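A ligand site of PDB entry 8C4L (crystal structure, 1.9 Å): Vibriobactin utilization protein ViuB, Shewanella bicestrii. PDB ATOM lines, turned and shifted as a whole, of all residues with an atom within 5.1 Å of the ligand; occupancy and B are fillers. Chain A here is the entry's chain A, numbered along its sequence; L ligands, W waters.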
ATOM      1  N   TYR A  42     -17.241  26.596 -20.393  1.00  0.00           N
ATOM      2  CA  TYR A  42     -16.088  26.085 -19.657  1.00  0.00           C
ATOM      3  C   TYR A  42     -15.650  24.757 -20.224  1.00  0.00           C
ATOM      4  O   TYR A  42     -16.440  24.011 -20.811  1.00  0.00           O
ATOM      5  CB  TYR A  42     -16.374  25.954 -18.163  1.00  0.00           C
ATOM      6  CG  TYR A  42     -17.295  24.825 -17.779  1.00  0.00           C
ATOM      7  CD1 TYR A  42     -16.867  23.485 -17.781  1.00  0.00           C
ATOM      8  CD2 TYR A  42     -18.585  25.085 -17.303  1.00  0.00           C
ATOM      9  CE1 TYR A  42     -17.715  22.426 -17.370  1.00  0.00           C
ATOM     10  CE2 TYR A  42     -19.443  24.037 -16.900  1.00  0.00           C
ATOM     11  CZ  TYR A  42     -18.989  22.719 -16.929  1.00  0.00           C
ATOM     12  OH  TYR A  42     -19.839  21.693 -16.529  1.00  0.00           O
ATOM     13  N   ARG A  58      -9.088  20.633 -13.996  1.00  0.00           N
ATOM     14  CA  ARG A  58      -9.150  22.052 -13.740  1.00  0.00           C
ATOM     15  C   ARG A  58     -10.065  22.723 -14.756  1.00  0.00           C
ATOM     16  O   ARG A  58     -10.012  22.405 -15.953  1.00  0.00           O
ATOM     17  CB  ARG A  58      -7.754  22.656 -13.805  1.00  0.00           C
ATOM     18  CG  ARG A  58      -6.806  22.069 -12.768  1.00  0.00           C
ATOM     19  CD  ARG A  58      -7.217  22.457 -11.385  1.00  0.00           C
ATOM     20  NE  ARG A  58      -6.243  22.112 -10.366  1.00  0.00           N
ATOM     21  CZ  ARG A  58      -6.350  21.068  -9.552  1.00  0.00           C
ATOM     22  NH1 ARG A  58      -7.316  20.189  -9.661  1.00  0.00           N
ATOM     23  NH2 ARG A  58      -5.493  20.948  -8.543  1.00  0.00           N
ATOM     24  N   THR A  59     -10.837  23.698 -14.296  1.00  0.00           N
ATOM     25  CA  THR A  59     -11.844  24.369 -15.105  1.00  0.00           C
ATOM     26  C   THR A  59     -11.318  25.678 -15.697  1.00  0.00           C
ATOM     27  O   THR A  59     -10.804  26.546 -14.971  1.00  0.00           O
ATOM     28  CB  THR A  59     -13.085  24.636 -14.253  1.00  0.00           C
ATOM     29  OG1 THR A  59     -13.478  23.414 -13.635  1.00  0.00           O
ATOM     30  CG2 THR A  59     -14.239  25.167 -15.116  1.00  0.00           C
ATOM     31  N   TYR A  60     -11.484  25.825 -17.012  1.00  0.00           N
ATOM     32  CA  TYR A  60     -11.042  27.024 -17.718  1.00  0.00           C
ATOM     33  C   TYR A  60     -12.141  27.433 -18.703  1.00  0.00           C
ATOM     34  O   TYR A  60     -13.048  26.657 -19.020  1.00  0.00           O
ATOM     35  CB  TYR A  60      -9.704  26.776 -18.451  1.00  0.00           C
ATOM     36  CG  TYR A  60      -8.562  26.865 -17.464  1.00  0.00           C
ATOM     37  CD1 TYR A  60      -7.928  28.075 -17.215  1.00  0.00           C
ATOM     38  CD2 TYR A  60      -8.205  25.771 -16.709  1.00  0.00           C
ATOM     39  CE1 TYR A  60      -6.930  28.165 -16.277  1.00  0.00           C
ATOM     40  CE2 TYR A  60      -7.195  25.857 -15.770  1.00  0.00           C
ATOM     41  CZ  TYR A  60      -6.566  27.058 -15.561  1.00  0.00           C
ATOM     42  OH  TYR A  60      -5.593  27.144 -14.624  1.00  0.00           O
ATOM     43  N   THR A  61     -12.044  28.660 -19.156  1.00  0.00           N
ATOM     44  CA  THR A  61     -13.008  29.249 -20.054  1.00  0.00           C
ATOM     45  C   THR A  61     -12.485  29.217 -21.482  1.00  0.00           C
ATOM     46  O   THR A  61     -11.295  29.418 -21.733  1.00  0.00           O
ATOM     47  CB  THR A  61     -13.289  30.690 -19.656  1.00  0.00           C
ATOM     48  OG1 THR A  61     -13.695  30.764 -18.282  1.00  0.00           O
ATOM     49  CG2 THR A  61     -14.350  31.277 -20.512  1.00  0.00           C
ATOM     50  N   VAL A  72      -7.443  29.523 -24.733  1.00  0.00           N
ATOM     51  CA  VAL A  72      -7.717  29.490 -23.316  1.00  0.00           C
ATOM     52  C   VAL A  72      -6.718  30.393 -22.646  1.00  0.00           C
ATOM     53  O   VAL A  72      -5.521  30.290 -22.896  1.00  0.00           O
ATOM     54  CB  VAL A  72      -7.609  28.065 -22.757  1.00  0.00           C
ATOM     55  CG1 VAL A  72      -7.927  28.050 -21.239  1.00  0.00           C
ATOM     56  CG2 VAL A  72      -8.535  27.118 -23.538  1.00  0.00           C
ATOM     57  N   ASP A  73      -7.213  31.284 -21.780  1.00  0.00           N
ATOM     58  CA  ASP A  73      -6.416  32.284 -21.091  1.00  0.00           C
ATOM     59  C   ASP A  73      -6.193  31.822 -19.646  1.00  0.00           C
ATOM     60  O   ASP A  73      -7.165  31.559 -18.919  1.00  0.00           O
ATOM     61  CB  ASP A  73      -7.110  33.652 -21.109  1.00  0.00           C
ATOM     62  CG  ASP A  73      -7.063  34.353 -22.482  1.00  0.00           C
ATOM     63  OD1 ASP A  73      -6.594  33.722 -23.459  1.00  0.00           O
ATOM     64  OD2 ASP A  73      -7.511  35.543 -22.559  1.00  0.00           O
ATOM     65  N   PHE A  74      -4.926  31.730 -19.243  1.00  0.00           N
ATOM     66  CA  PHE A  74      -4.522  31.248 -17.925  1.00  0.00           C
ATOM     67  C   PHE A  74      -3.995  32.407 -17.103  1.00  0.00           C
ATOM     68  O   PHE A  74      -3.012  33.055 -17.499  1.00  0.00           O
ATOM     69  CB  PHE A  74      -3.422  30.189 -18.028  1.00  0.00           C
ATOM     70  CG  PHE A  74      -3.840  28.909 -18.669  1.00  0.00           C
ATOM     71  CD1 PHE A  74      -4.029  28.838 -20.030  1.00  0.00           C
ATOM     72  CD2 PHE A  74      -4.022  27.785 -17.893  1.00  0.00           C
ATOM     73  CE1 PHE A  74      -4.398  27.649 -20.620  1.00  0.00           C
ATOM     74  CE2 PHE A  74      -4.411  26.588 -18.471  1.00  0.00           C
ATOM     75  CZ  PHE A  74      -4.583  26.516 -19.853  1.00  0.00           C
ATOM     76  N   VAL A  75      -4.577  32.601 -15.925  1.00  0.00           N
ATOM     77  CA  VAL A  75      -3.983  33.502 -14.942  1.00  0.00           C
ATOM     78  C   VAL A  75      -2.751  32.850 -14.335  1.00  0.00           C
ATOM     79  O   VAL A  75      -2.806  31.706 -13.871  1.00  0.00           O
ATOM     80  CB  VAL A  75      -4.968  33.838 -13.823  1.00  0.00           C
ATOM     81  CG1 VAL A  75      -4.294  34.768 -12.806  1.00  0.00           C
ATOM     82  CG2 VAL A  75      -6.201  34.470 -14.421  1.00  0.00           C
ATOM     83  N   HIS A  77      -1.157  32.700 -11.601  1.00  0.00           N
ATOM     84  CA  HIS A  77      -1.476  33.065 -10.245  1.00  0.00           C
ATOM     85  C   HIS A  77      -0.385  32.653  -9.266  1.00  0.00           C
ATOM     86  O   HIS A  77       0.402  31.729  -9.510  1.00  0.00           O
ATOM     87  CB  HIS A  77      -2.806  32.423  -9.823  1.00  0.00           C
ATOM     88  CG  HIS A  77      -2.837  30.932  -9.941  1.00  0.00           C
ATOM     89  ND1 HIS A  77      -2.332  30.104  -8.967  1.00  0.00           N
ATOM     90  CD2 HIS A  77      -3.327  30.118 -10.910  1.00  0.00           C
ATOM     91  CE1 HIS A  77      -2.506  28.843  -9.323  1.00  0.00           C
ATOM     92  NE2 HIS A  77      -3.109  28.831 -10.505  1.00  0.00           N
ATOM     93  N   ASP A  78      -0.386  33.343  -8.126  1.00  0.00           N
ATOM     94  CA  ASP A  78       0.395  32.945  -6.966  1.00  0.00           C
ATOM     95  C   ASP A  78       0.086  31.507  -6.605  1.00  0.00           C
ATOM     96  O   ASP A  78      -1.042  31.045  -6.749  1.00  0.00           O
ATOM     97  CB  ASP A  78       0.075  33.842  -5.769  1.00  0.00           C
ATOM     98  CG  ASP A  78       1.061  34.994  -5.549  1.00  0.00           C
ATOM     99  OD1 ASP A  78       2.135  35.022  -6.223  1.00  0.00           O
ATOM    100  OD2 ASP A  78       0.774  35.842  -4.647  1.00  0.00           O
ATOM    101  N   THR A  79       1.128  30.783  -6.195  1.00  0.00           N
ATOM    102  CA  THR A  79       0.985  29.399  -5.751  1.00  0.00           C
ATOM    103  C   THR A  79       0.558  28.493  -6.883  1.00  0.00           C
ATOM    104  O   THR A  79      -0.612  28.120  -6.975  1.00  0.00           O
ATOM    105  CB  THR A  79       0.010  29.300  -4.578  1.00  0.00           C
ATOM    106  OG1 THR A  79       0.433  30.219  -3.567  1.00  0.00           O
ATOM    107  CG2 THR A  79       0.094  27.886  -3.976  1.00  0.00           C
ATOM    108  N   ASP A  80       1.517  28.130  -7.734  1.00  0.00           N
ATOM    109  CA  ASP A  80       1.228  27.310  -8.896  1.00  0.00           C
ATOM    110  C   ASP A  80       0.452  26.054  -8.511  1.00  0.00           C
ATOM    111  O   ASP A  80       0.687  25.456  -7.452  1.00  0.00           O
ATOM    112  CB  ASP A  80       2.522  26.921  -9.595  1.00  0.00           C
ATOM    113  CG  ASP A  80       2.911  27.873 -10.706  1.00  0.00           C
ATOM    114  OD1 ASP A  80       2.026  28.390 -11.405  1.00  0.00           O
ATOM    115  OD2 ASP A  80       4.115  28.119 -10.894  1.00  0.00           O
ATOM    116  N   GLY A  81      -0.497  25.696  -9.363  1.00  0.00           N
ATOM    117  CA  GLY A  81      -1.099  24.398  -9.377  1.00  0.00           C
ATOM    118  C   GLY A  81      -0.725  23.689 -10.675  1.00  0.00           C
ATOM    119  O   GLY A  81       0.046  24.213 -11.489  1.00  0.00           O
ATOM    120  N   PRO A  82      -1.268  22.497 -10.881  1.00  0.00           N
ATOM    121  CA  PRO A  82      -0.940  21.764 -12.107  1.00  0.00           C
ATOM    122  C   PRO A  82      -1.274  22.533 -13.366  1.00  0.00           C
ATOM    123  O   PRO A  82      -0.509  22.442 -14.335  1.00  0.00           O
ATOM    124  CB  PRO A  82      -1.764  20.479 -11.988  1.00  0.00           C
ATOM    125  CG  PRO A  82      -2.810  20.752 -10.985  1.00  0.00           C
ATOM    126  CD  PRO A  82      -2.185  21.735 -10.027  1.00  0.00           C
ATOM    127  N   ALA A  83      -2.360  23.310 -13.382  1.00  0.00           N
ATOM    128  CA  ALA A  83      -2.734  23.939 -14.648  1.00  0.00           C
ATOM    129  C   ALA A  83      -1.834  25.124 -14.944  1.00  0.00           C
ATOM    130  O   ALA A  83      -1.390  25.306 -16.085  1.00  0.00           O
ATOM    131  CB  ALA A  83      -4.202  24.380 -14.631  1.00  0.00           C
ATOM    132  N   SER A  84      -1.610  25.981 -13.950  1.00  0.00           N
ATOM    133  CA  SER A  84      -0.793  27.160 -14.202  1.00  0.00           C
ATOM    134  C   SER A  84       0.652  26.781 -14.490  1.00  0.00           C
ATOM    135  O   SER A  84       1.275  27.373 -15.377  1.00  0.00           O
ATOM    136  CB  SER A  84      -0.886  28.158 -13.040  1.00  0.00           C
ATOM    137  OG  SER A  84      -0.497  27.606 -11.810  1.00  0.00           O
ATOM    138  N   MET A 120      -9.401  38.170 -12.401  1.00  0.00           N
ATOM    139  CA  MET A 120      -8.778  37.746 -13.636  1.00  0.00           C
ATOM    140  C   MET A 120      -9.242  36.378 -14.077  1.00  0.00           C
ATOM    141  O   MET A 120      -9.196  36.078 -15.289  1.00  0.00           O
ATOM    142  CB  MET A 120      -7.241  37.797 -13.513  1.00  0.00           C
ATOM    143  CG  MET A 120      -6.737  39.211 -13.607  1.00  0.00           C
ATOM    144  SD  MET A 120      -4.980  39.393 -13.437  1.00  0.00           S
ATOM    145  CE  MET A 120      -4.377  38.780 -14.992  1.00  0.00           C
ATOM    146  N   THR A 121      -9.705  35.514 -13.162  1.00  0.00           N
ATOM    147  CA  THR A 121     -10.213  34.231 -13.614  1.00  0.00           C
ATOM    148  C   THR A 121     -11.471  34.385 -14.433  1.00  0.00           C
ATOM    149  O   THR A 121     -11.805  33.496 -15.216  1.00  0.00           O
ATOM    150  CB  THR A 121     -10.484  33.289 -12.440  1.00  0.00           C
ATOM    151  OG1 THR A 121     -11.494  33.831 -11.599  1.00  0.00           O
ATOM    152  CG2 THR A 121      -9.246  33.044 -11.658  1.00  0.00           C
ATOM    153  N   PRO A 124     -11.713  36.343 -18.993  1.00  0.00           N
ATOM    154  CA  PRO A 124     -12.069  35.783 -20.300  1.00  0.00           C
ATOM    155  C   PRO A 124     -13.564  35.764 -20.561  1.00  0.00           C
ATOM    156  O   PRO A 124     -14.011  36.148 -21.658  1.00  0.00           O
ATOM    157  CB  PRO A 124     -11.446  34.374 -20.238  1.00  0.00           C
ATOM    158  CG  PRO A 124     -10.228  34.552 -19.321  1.00  0.00           C
ATOM    159  CD  PRO A 124     -10.772  35.478 -18.253  1.00  0.00           C
ATOM    160  N   SER A 224     -18.626  31.460  -7.780  1.00  0.00           N
ATOM    161  CA  SER A 224     -17.269  31.384  -7.262  1.00  0.00           C
ATOM    162  C   SER A 224     -16.443  30.582  -8.260  1.00  0.00           C
ATOM    163  O   SER A 224     -16.814  29.465  -8.623  1.00  0.00           O
ATOM    164  CB  SER A 224     -17.267  30.735  -5.890  1.00  0.00           C
ATOM    165  OG  SER A 224     -15.947  30.573  -5.371  1.00  0.00           O
ATOM    166  N   TYR A 225     -15.345  31.162  -8.743  1.00  0.00           N
ATOM    167  CA  TYR A 225     -14.432  30.484  -9.670  1.00  0.00           C
ATOM    168  C   TYR A 225     -13.204  29.890  -8.980  1.00  0.00           C
ATOM    169  O   TYR A 225     -12.585  28.964  -9.533  1.00  0.00           O
ATOM    170  CB  TYR A 225     -13.974  31.443 -10.772  1.00  0.00           C
ATOM    171  CG  TYR A 225     -14.905  31.562 -11.990  1.00  0.00           C
ATOM    172  CD1 TYR A 225     -16.221  31.089 -11.967  1.00  0.00           C
ATOM    173  CD2 TYR A 225     -14.458  32.122 -13.145  1.00  0.00           C
ATOM    174  CE1 TYR A 225     -17.022  31.209 -13.067  1.00  0.00           C
ATOM    175  CE2 TYR A 225     -15.251  32.245 -14.239  1.00  0.00           C
ATOM    176  CZ  TYR A 225     -16.514  31.777 -14.202  1.00  0.00           C
ATOM    177  OH  TYR A 225     -17.297  31.894 -15.341  1.00  0.00           O
ATOM    178  N   TRP A 226     -12.864  30.326  -7.770  1.00  0.00           N
ATOM    179  CA  TRP A 226     -11.760  29.742  -7.024  1.00  0.00           C
ATOM    180  C   TRP A 226     -11.864  30.256  -5.588  1.00  0.00           C
ATOM    181  O   TRP A 226     -12.681  31.135  -5.284  1.00  0.00           O
ATOM    182  CB  TRP A 226     -10.397  30.078  -7.665  1.00  0.00           C
ATOM    183  CG  TRP A 226     -10.017  31.536  -7.598  1.00  0.00           C
ATOM    184  CD1 TRP A 226     -10.527  32.560  -8.343  1.00  0.00           C
ATOM    185  CD2 TRP A 226      -9.037  32.121  -6.732  1.00  0.00           C
ATOM    186  NE1 TRP A 226      -9.939  33.738  -7.985  1.00  0.00           N
ATOM    187  CE2 TRP A 226      -9.017  33.495  -6.992  1.00  0.00           C
ATOM    188  CE3 TRP A 226      -8.188  31.601  -5.746  1.00  0.00           C
ATOM    189  CZ2 TRP A 226      -8.202  34.377  -6.293  1.00  0.00           C
ATOM    190  CZ3 TRP A 226      -7.360  32.466  -5.073  1.00  0.00           C
ATOM    191  CH2 TRP A 226      -7.357  33.824  -5.356  1.00  0.00           C
ATOM    192  N   LYS A 227     -11.013  29.721  -4.717  1.00  0.00           N
ATOM    193  CA  LYS A 227     -10.950  30.195  -3.348  1.00  0.00           C
ATOM    194  C   LYS A 227      -9.520  30.133  -2.829  1.00  0.00           C
ATOM    195  O   LYS A 227      -8.811  29.131  -3.022  1.00  0.00           O
ATOM    196  CB  LYS A 227     -11.839  29.385  -2.425  1.00  0.00           C
ATOM    197  CG  LYS A 227     -11.843  29.873  -0.955  1.00  0.00           C
ATOM    198  CD  LYS A 227     -12.865  29.097  -0.146  1.00  0.00           C
ATOM    199  CE  LYS A 227     -13.182  29.692   1.228  1.00  0.00           C
ATOM    200  NZ  LYS A 227     -11.969  29.815   2.090  1.00  0.00           N
ATOM    201  N   ILE A 228      -9.143  31.205  -2.129  1.00  0.00           N
ATOM    202  CA  ILE A 228      -7.818  31.310  -1.511  1.00  0.00           C
ATOM    203  C   ILE A 228      -7.511  30.075  -0.681  1.00  0.00           C
ATOM    204  O   ILE A 228      -8.329  29.629   0.128  1.00  0.00           O
ATOM    205  CB  ILE A 228      -7.765  32.584  -0.659  1.00  0.00           C
ATOM    206  CG1 ILE A 228      -7.887  33.834  -1.552  1.00  0.00           C
ATOM    207  CG2 ILE A 228      -6.507  32.604   0.153  1.00  0.00           C
ATOM    208  CD1 ILE A 228      -8.366  35.093  -0.763  1.00  0.00           C
ATOM    209  N   GLY A 229      -6.320  29.512  -0.879  1.00  0.00           N
ATOM    210  CA  GLY A 229      -5.900  28.368  -0.101  1.00  0.00           C
ATOM    211  C   GLY A 229      -6.478  27.038  -0.542  1.00  0.00           C
ATOM    212  O   GLY A 229      -6.060  25.998  -0.029  1.00  0.00           O
ATOM    213  N   CYS A 230      -7.399  27.029  -1.514  1.00  0.00           N
ATOM    214  CA  CYS A 230      -8.039  25.811  -1.990  1.00  0.00           C
ATOM    215  C   CYS A 230      -7.584  25.476  -3.403  1.00  0.00           C
ATOM    216  O   CYS A 230      -7.575  26.344  -4.285  1.00  0.00           O
ATOM    217  CB  CYS A 230      -9.567  25.937  -1.998  1.00  0.00           C
ATOM    218  SG  CYS A 230     -10.276  26.178  -0.365  1.00  0.00           S
ATOM    219  N   ASN A 231      -7.216  24.217  -3.617  1.00  0.00           N
ATOM    220  CA  ASN A 231      -7.131  23.723  -4.969  1.00  0.00           C
ATOM    221  C   ASN A 231      -8.557  23.476  -5.463  1.00  0.00           C
ATOM    222  O   ASN A 231      -9.509  23.546  -4.700  1.00  0.00           O
ATOM    223  CB  ASN A 231      -6.267  22.463  -5.050  1.00  0.00           C
ATOM    224  CG  ASN A 231      -6.805  21.300  -4.251  1.00  0.00           C
ATOM    225  OD1 ASN A 231      -8.009  21.048  -4.214  1.00  0.00           O
ATOM    226  ND2 ASN A 231      -5.905  20.599  -3.577  1.00  0.00           N
ATOM    227  N   GLU A 232      -8.704  23.219  -6.764  1.00  0.00           N
ATOM    228  CA  GLU A 232     -10.051  23.221  -7.332  1.00  0.00           C
ATOM    229  C   GLU A 232     -10.950  22.164  -6.666  1.00  0.00           C
ATOM    230  O   GLU A 232     -12.140  22.408  -6.452  1.00  0.00           O
ATOM    231  CB  GLU A 232      -9.986  23.030  -8.839  1.00  0.00           C
ATOM    232  CG  GLU A 232     -11.350  22.774  -9.445  1.00  0.00           C
ATOM    233  CD  GLU A 232     -11.434  23.081 -10.919  1.00  0.00           C
ATOM    234  OE1 GLU A 232     -10.612  23.910 -11.403  1.00  0.00           O
ATOM    235  OE2 GLU A 232     -12.334  22.531 -11.600  1.00  0.00           O
ATOM    236  N   LYS A 239     -18.049  25.554  -2.693  1.00  0.00           N
ATOM    237  CA  LYS A 239     -18.938  26.214  -3.635  1.00  0.00           C
ATOM    238  C   LYS A 239     -20.297  25.532  -3.671  1.00  0.00           C
ATOM    239  O   LYS A 239     -21.328  26.199  -3.694  1.00  0.00           O
ATOM    240  CB  LYS A 239     -18.300  26.247  -5.021  1.00  0.00           C
ATOM    241  CG  LYS A 239     -19.155  26.874  -6.096  1.00  0.00           C
ATOM    242  CD  LYS A 239     -18.472  26.869  -7.455  1.00  0.00           C
ATOM    243  CE  LYS A 239     -19.392  27.462  -8.533  1.00  0.00           C
ATOM    244  NZ  LYS A 239     -18.694  27.509  -9.865  1.00  0.00           N
HETATM  245  P1  LIG L   1      -5.134  24.645  -8.100  1.00  0.00           P
HETATM  246  O1  LIG L   1      -4.256  23.436  -7.966  1.00  0.00           O
HETATM  247  O2  LIG L   1      -6.620  24.491  -8.196  1.00  0.00           O
HETATM  248  O3  LIG L   1      -4.883  25.551  -6.873  1.00  0.00           O
HETATM  249  C1  LIG L   1      -3.534  25.795  -6.430  1.00  0.00           C
HETATM  250  C2  LIG L   1      -3.413  26.982  -5.530  1.00  0.00           C
HETATM  251  O4  LIG L   1      -3.500  28.193  -6.314  1.00  0.00           O
HETATM  252  C3  LIG L   1      -4.464  27.096  -4.434  1.00  0.00           C
HETATM  253  O5  LIG L   1      -3.821  27.536  -3.232  1.00  0.00           O
HETATM  254  C4  LIG L   1      -5.454  28.114  -5.005  1.00  0.00           C
HETATM  255  O6  LIG L   1      -6.158  28.839  -3.998  1.00  0.00           O
HETATM  256  C5  LIG L   1      -4.511  29.020  -5.783  1.00  0.00           C
HETATM  257  N1  LIG L   1      -5.164  29.720  -6.901  1.00  0.00           N
HETATM  258  C6  LIG L   1      -5.928  29.172  -7.897  1.00  0.00           C
HETATM  259  N2  LIG L   1      -6.369  30.046  -8.770  1.00  0.00           N
HETATM  260  C7  LIG L   1      -5.845  31.244  -8.319  1.00  0.00           C
HETATM  261  C8  LIG L   1      -5.937  32.559  -8.816  1.00  0.00           C
HETATM  262  N3  LIG L   1      -6.626  32.877  -9.909  1.00  0.00           N
HETATM  263  N4  LIG L   1      -5.306  33.538  -8.121  1.00  0.00           N
HETATM  264  C9  LIG L   1      -4.629  33.214  -7.010  1.00  0.00           C
HETATM  265  N5  LIG L   1      -4.456  32.017  -6.465  1.00  0.00           N
HETATM  266  C10 LIG L   1      -5.109  31.064  -7.160  1.00  0.00           C
HETATM  267  N6  LIG L   1      -9.049  30.533 -14.355  1.00  0.00           N
HETATM  268  C11 LIG L   1      -8.290  31.072 -15.348  1.00  0.00           C
HETATM  269  O7  LIG L   1      -7.131  31.406 -15.138  1.00  0.00           O
HETATM  270  N7  LIG L   1      -8.822  31.196 -16.615  1.00  0.00           N
HETATM  271  C12 LIG L   1     -10.102  30.823 -16.990  1.00  0.00           C
HETATM  272  O8  LIG L   1     -10.490  30.989 -18.139  1.00  0.00           O
HETATM  273  C13 LIG L   1     -10.900  30.306 -15.920  1.00  0.00           C
HETATM  274  N8  LIG L   1     -12.138  29.984 -16.184  1.00  0.00           N
HETATM  275  C14 LIG L   1     -12.883  29.409 -15.160  1.00  0.00           C
HETATM  276  C15 LIG L   1     -14.207  29.034 -15.425  1.00  0.00           C
HETATM  277  C16 LIG L   1     -15.001  28.459 -14.439  1.00  0.00           C
HETATM  278  C17 LIG L   1     -16.403  28.041 -14.736  1.00  0.00           C
HETATM  279  C18 LIG L   1     -14.467  28.257 -13.158  1.00  0.00           C
HETATM  280  C19 LIG L   1     -15.317  27.660 -12.071  1.00  0.00           C
HETATM  281  C20 LIG L   1     -13.156  28.637 -12.894  1.00  0.00           C
HETATM  282  C21 LIG L   1     -12.365  29.203 -13.891  1.00  0.00           C
HETATM  283  N9  LIG L   1     -11.029  29.584 -13.644  1.00  0.00           N
HETATM  284  C22 LIG L   1     -10.275  30.150 -14.642  1.00  0.00           C
HETATM  285  C23 LIG L   1     -10.413  29.400 -12.309  1.00  0.00           C
HETATM  286  C24 LIG L   1      -9.496  28.170 -12.251  1.00  0.00           C
HETATM  287  O9  LIG L   1     -10.276  26.985 -12.336  1.00  0.00           O
HETATM  288  C25 LIG L   1      -8.728  28.157 -10.931  1.00  0.00           C
HETATM  289  O10 LIG L   1      -7.860  29.282 -10.936  1.00  0.00           O
HETATM  290  C26 LIG L   1      -7.873  26.900 -10.678  1.00  0.00           C
HETATM  291  O11 LIG L   1      -7.702  26.758  -9.269  1.00  0.00           O
HETATM  292  C27 LIG L   1      -6.509  26.949 -11.334  1.00  0.00           C
HETATM  293  O12 LIG L   1      -5.933  25.620 -11.348  1.00  0.00           O
HETATM  294  P2  LIG L   1      -4.459  25.370 -10.857  1.00  0.00           P
HETATM  295  O13 LIG L   1      -4.158  23.905 -11.168  1.00  0.00           O
HETATM  296  O14 LIG L   1      -3.444  26.307 -11.385  1.00  0.00           O
HETATM  297  O15 LIG L   1      -4.582  25.574  -9.262  1.00  0.00           O
HETATM  298  O   HOH W   1      -2.673  25.303  -2.037  1.00  0.00           O
HETATM  299  O   HOH W   2      -3.942  30.122  -2.189  1.00  0.00           O
HETATM  300  O   HOH W   3     -12.060  26.404 -10.094  1.00  0.00           O
HETATM  301  O   HOH W   4      -9.813  31.482 -20.697  1.00  0.00           O
HETATM  302  O   HOH W   5      -9.997  26.385  -8.103  1.00  0.00           O
HETATM  303  O   HOH W   6      -6.496  30.752 -12.514  1.00  0.00           O
HETATM  304  O   HOH W   7      -4.526  29.557 -13.960  1.00  0.00           O
HETATM  305  O   HOH W   8      -7.227  35.963 -10.057  1.00  0.00           O
HETATM  306  O   HOH W   9     -16.790  25.240 -10.231  1.00  0.00           O
HETATM  307  O   HOH W  10      -5.000  36.194  -8.218  1.00  0.00           O
HETATM  308  O   HOH W  11      -2.594  22.299  -6.468  1.00  0.00           O
HETATM  309  O   HOH W  12      -3.046  32.196  -3.905  1.00  0.00           O
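NH2 of Arg 58 lies within salt-bridge range of O1 of the ligand (2.8 Å). The backbone NH of Gly 229 is in hydrogen-bond range of an oxygen (O6) of the ligand (3.2 Å). An oxygen (O14) of the ligand lies within hydrogen-bond range of a ring nitrogen (NE2) of His 77 (2.7 Å). N of Thr 61 lies within hydrogen-bond range of O8 of the ligand, at 3.0 Å. A nitrogen (N8) of the ligand sits at hydrogen-bond distance from the side-chain hydroxyl (OG1) of Thr 61 (2.7 Å). The backbone NH (N) of Ser 84 sits at hydrogen-bond distance from an oxygen (O14) of the ligand, 3.2 Å away. O13 of the ligand sits at hydrogen-bond distance from N of Ala 83 (2.9 Å). An oxygen (O9) of the ligand sits at hydrogen-bond distance from the side-chain carboxylate (OE1) of Glu 232. O9 of the ligand is in hydrogen-bond range of O of Thr 59, at 2.7 Å. O6 of the ligand lies within hydrogen-bond range of N of Cys 230 (3.3 Å). O of Lys 227 sits at hydrogen-bond distance from O6 of the ligand, 2.8 Å away. OG of Ser 84 sits at hydrogen-bond distance from O14 of the ligand, 3.2 Å away. An oxygen (O2) of the ligand lies within hydrogen-bond range of the backbone NH (N) of Glu 232. The backbone carbonyl oxygen (O) of Cys 230 sits close to an oxygen (O6) of the ligand, 2.9 Å away. The backbone NH of Val 75 sits at hydrogen-bond distance from an oxygen (O7) of the ligand. A nitrogen (N7) of the ligand lies within hydrogen-bond range of the backbone carbonyl oxygen (O) of Asp 73 (2.9 Å).
The backbone NH (N) of Gly 81 is in hydrogen-bond range of the side-chain hydroxyl (OG) of Ser 84 (3.1 Å). The side-chain hydroxyl of Thr 59 is in hydrogen-bond range of the side-chain carboxylate of Glu 232 (2.5 Å). ND1 of His 77 sits close to O of Thr 79 (3.3 Å). The backbone carbonyl oxygen (O) of Trp 226 is in hydrogen-bond range of the side-chain hydroxyl (OG) of Ser 224 (3.3 Å). The side-chain hydroxyl (OG) of Ser 84 is in hydrogen-bond range of a ring nitrogen (NE2) of His 77, 3.2 Å away. The side-chain hydroxyl (OG) of Ser 84 sits at hydrogen-bond distance from the side-chain carboxylate (OD1) of Asp 80, 2.7 Å away.
The backbone carbonyl oxygen of Thr 79 lies close to an oxygen (O4) of the ligand. The backbone nitrogen (N) of Pro 82 sits close to an oxygen (O13) of the ligand, at 3.2 Å. Tyr 60 touches the ligand (CD1 to N7, 3.3 Å). Phe 74 touches the ligand. Asp 78 touches the ligand. C of Gly 81 touches O13 of the ligand, at 3.5 Å. Thr 121 touches the ligand. CG of Pro 124 touches O8 of the ligand, 3.8 Å away. O of Tyr 225 touches C20 of the ligand (3.4 Å). Trp 226 touches the ligand. Ile 228 touches the ligand. Asn 231 touches the ligand (CA to O2, 3.4 Å). Within 4 Å of the ligand: Arg 58, Thr 59, Tyr 60, Thr 61, Asp 73, Phe 74, Val 75, His 77, Asp 78, Thr 79, Gly 81, Pro 82, Ala 83, Ser 84, Thr 121, Pro 124, Tyr 225, Trp 226, Lys 227, Ile 228, Gly 229, Cys 230, Asn 231 and Glu 232. Along chain A the residues within 4 Å of the ligand span positions 58 to 232.
Water W4 lies within hydrogen-bond range of O8 of the ligand, O of Thr 61 and N of Asp 73. Water W2 bridges the backbone NH of Gly 229 (2.8 Å) and an oxygen (O5) of the ligand (2.8 Å). Water W3 lies within hydrogen-bond range of O of Tyr 225 (2.7 Å), O9 of the ligand (2.9 Å) and OE1 of Glu 232 (3.2 Å). Water W7 lies within hydrogen-bond range of OH of Tyr 60 (2.7 Å), O of Val 75 (2.8 Å) and O7 of the ligand (3.4 Å).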
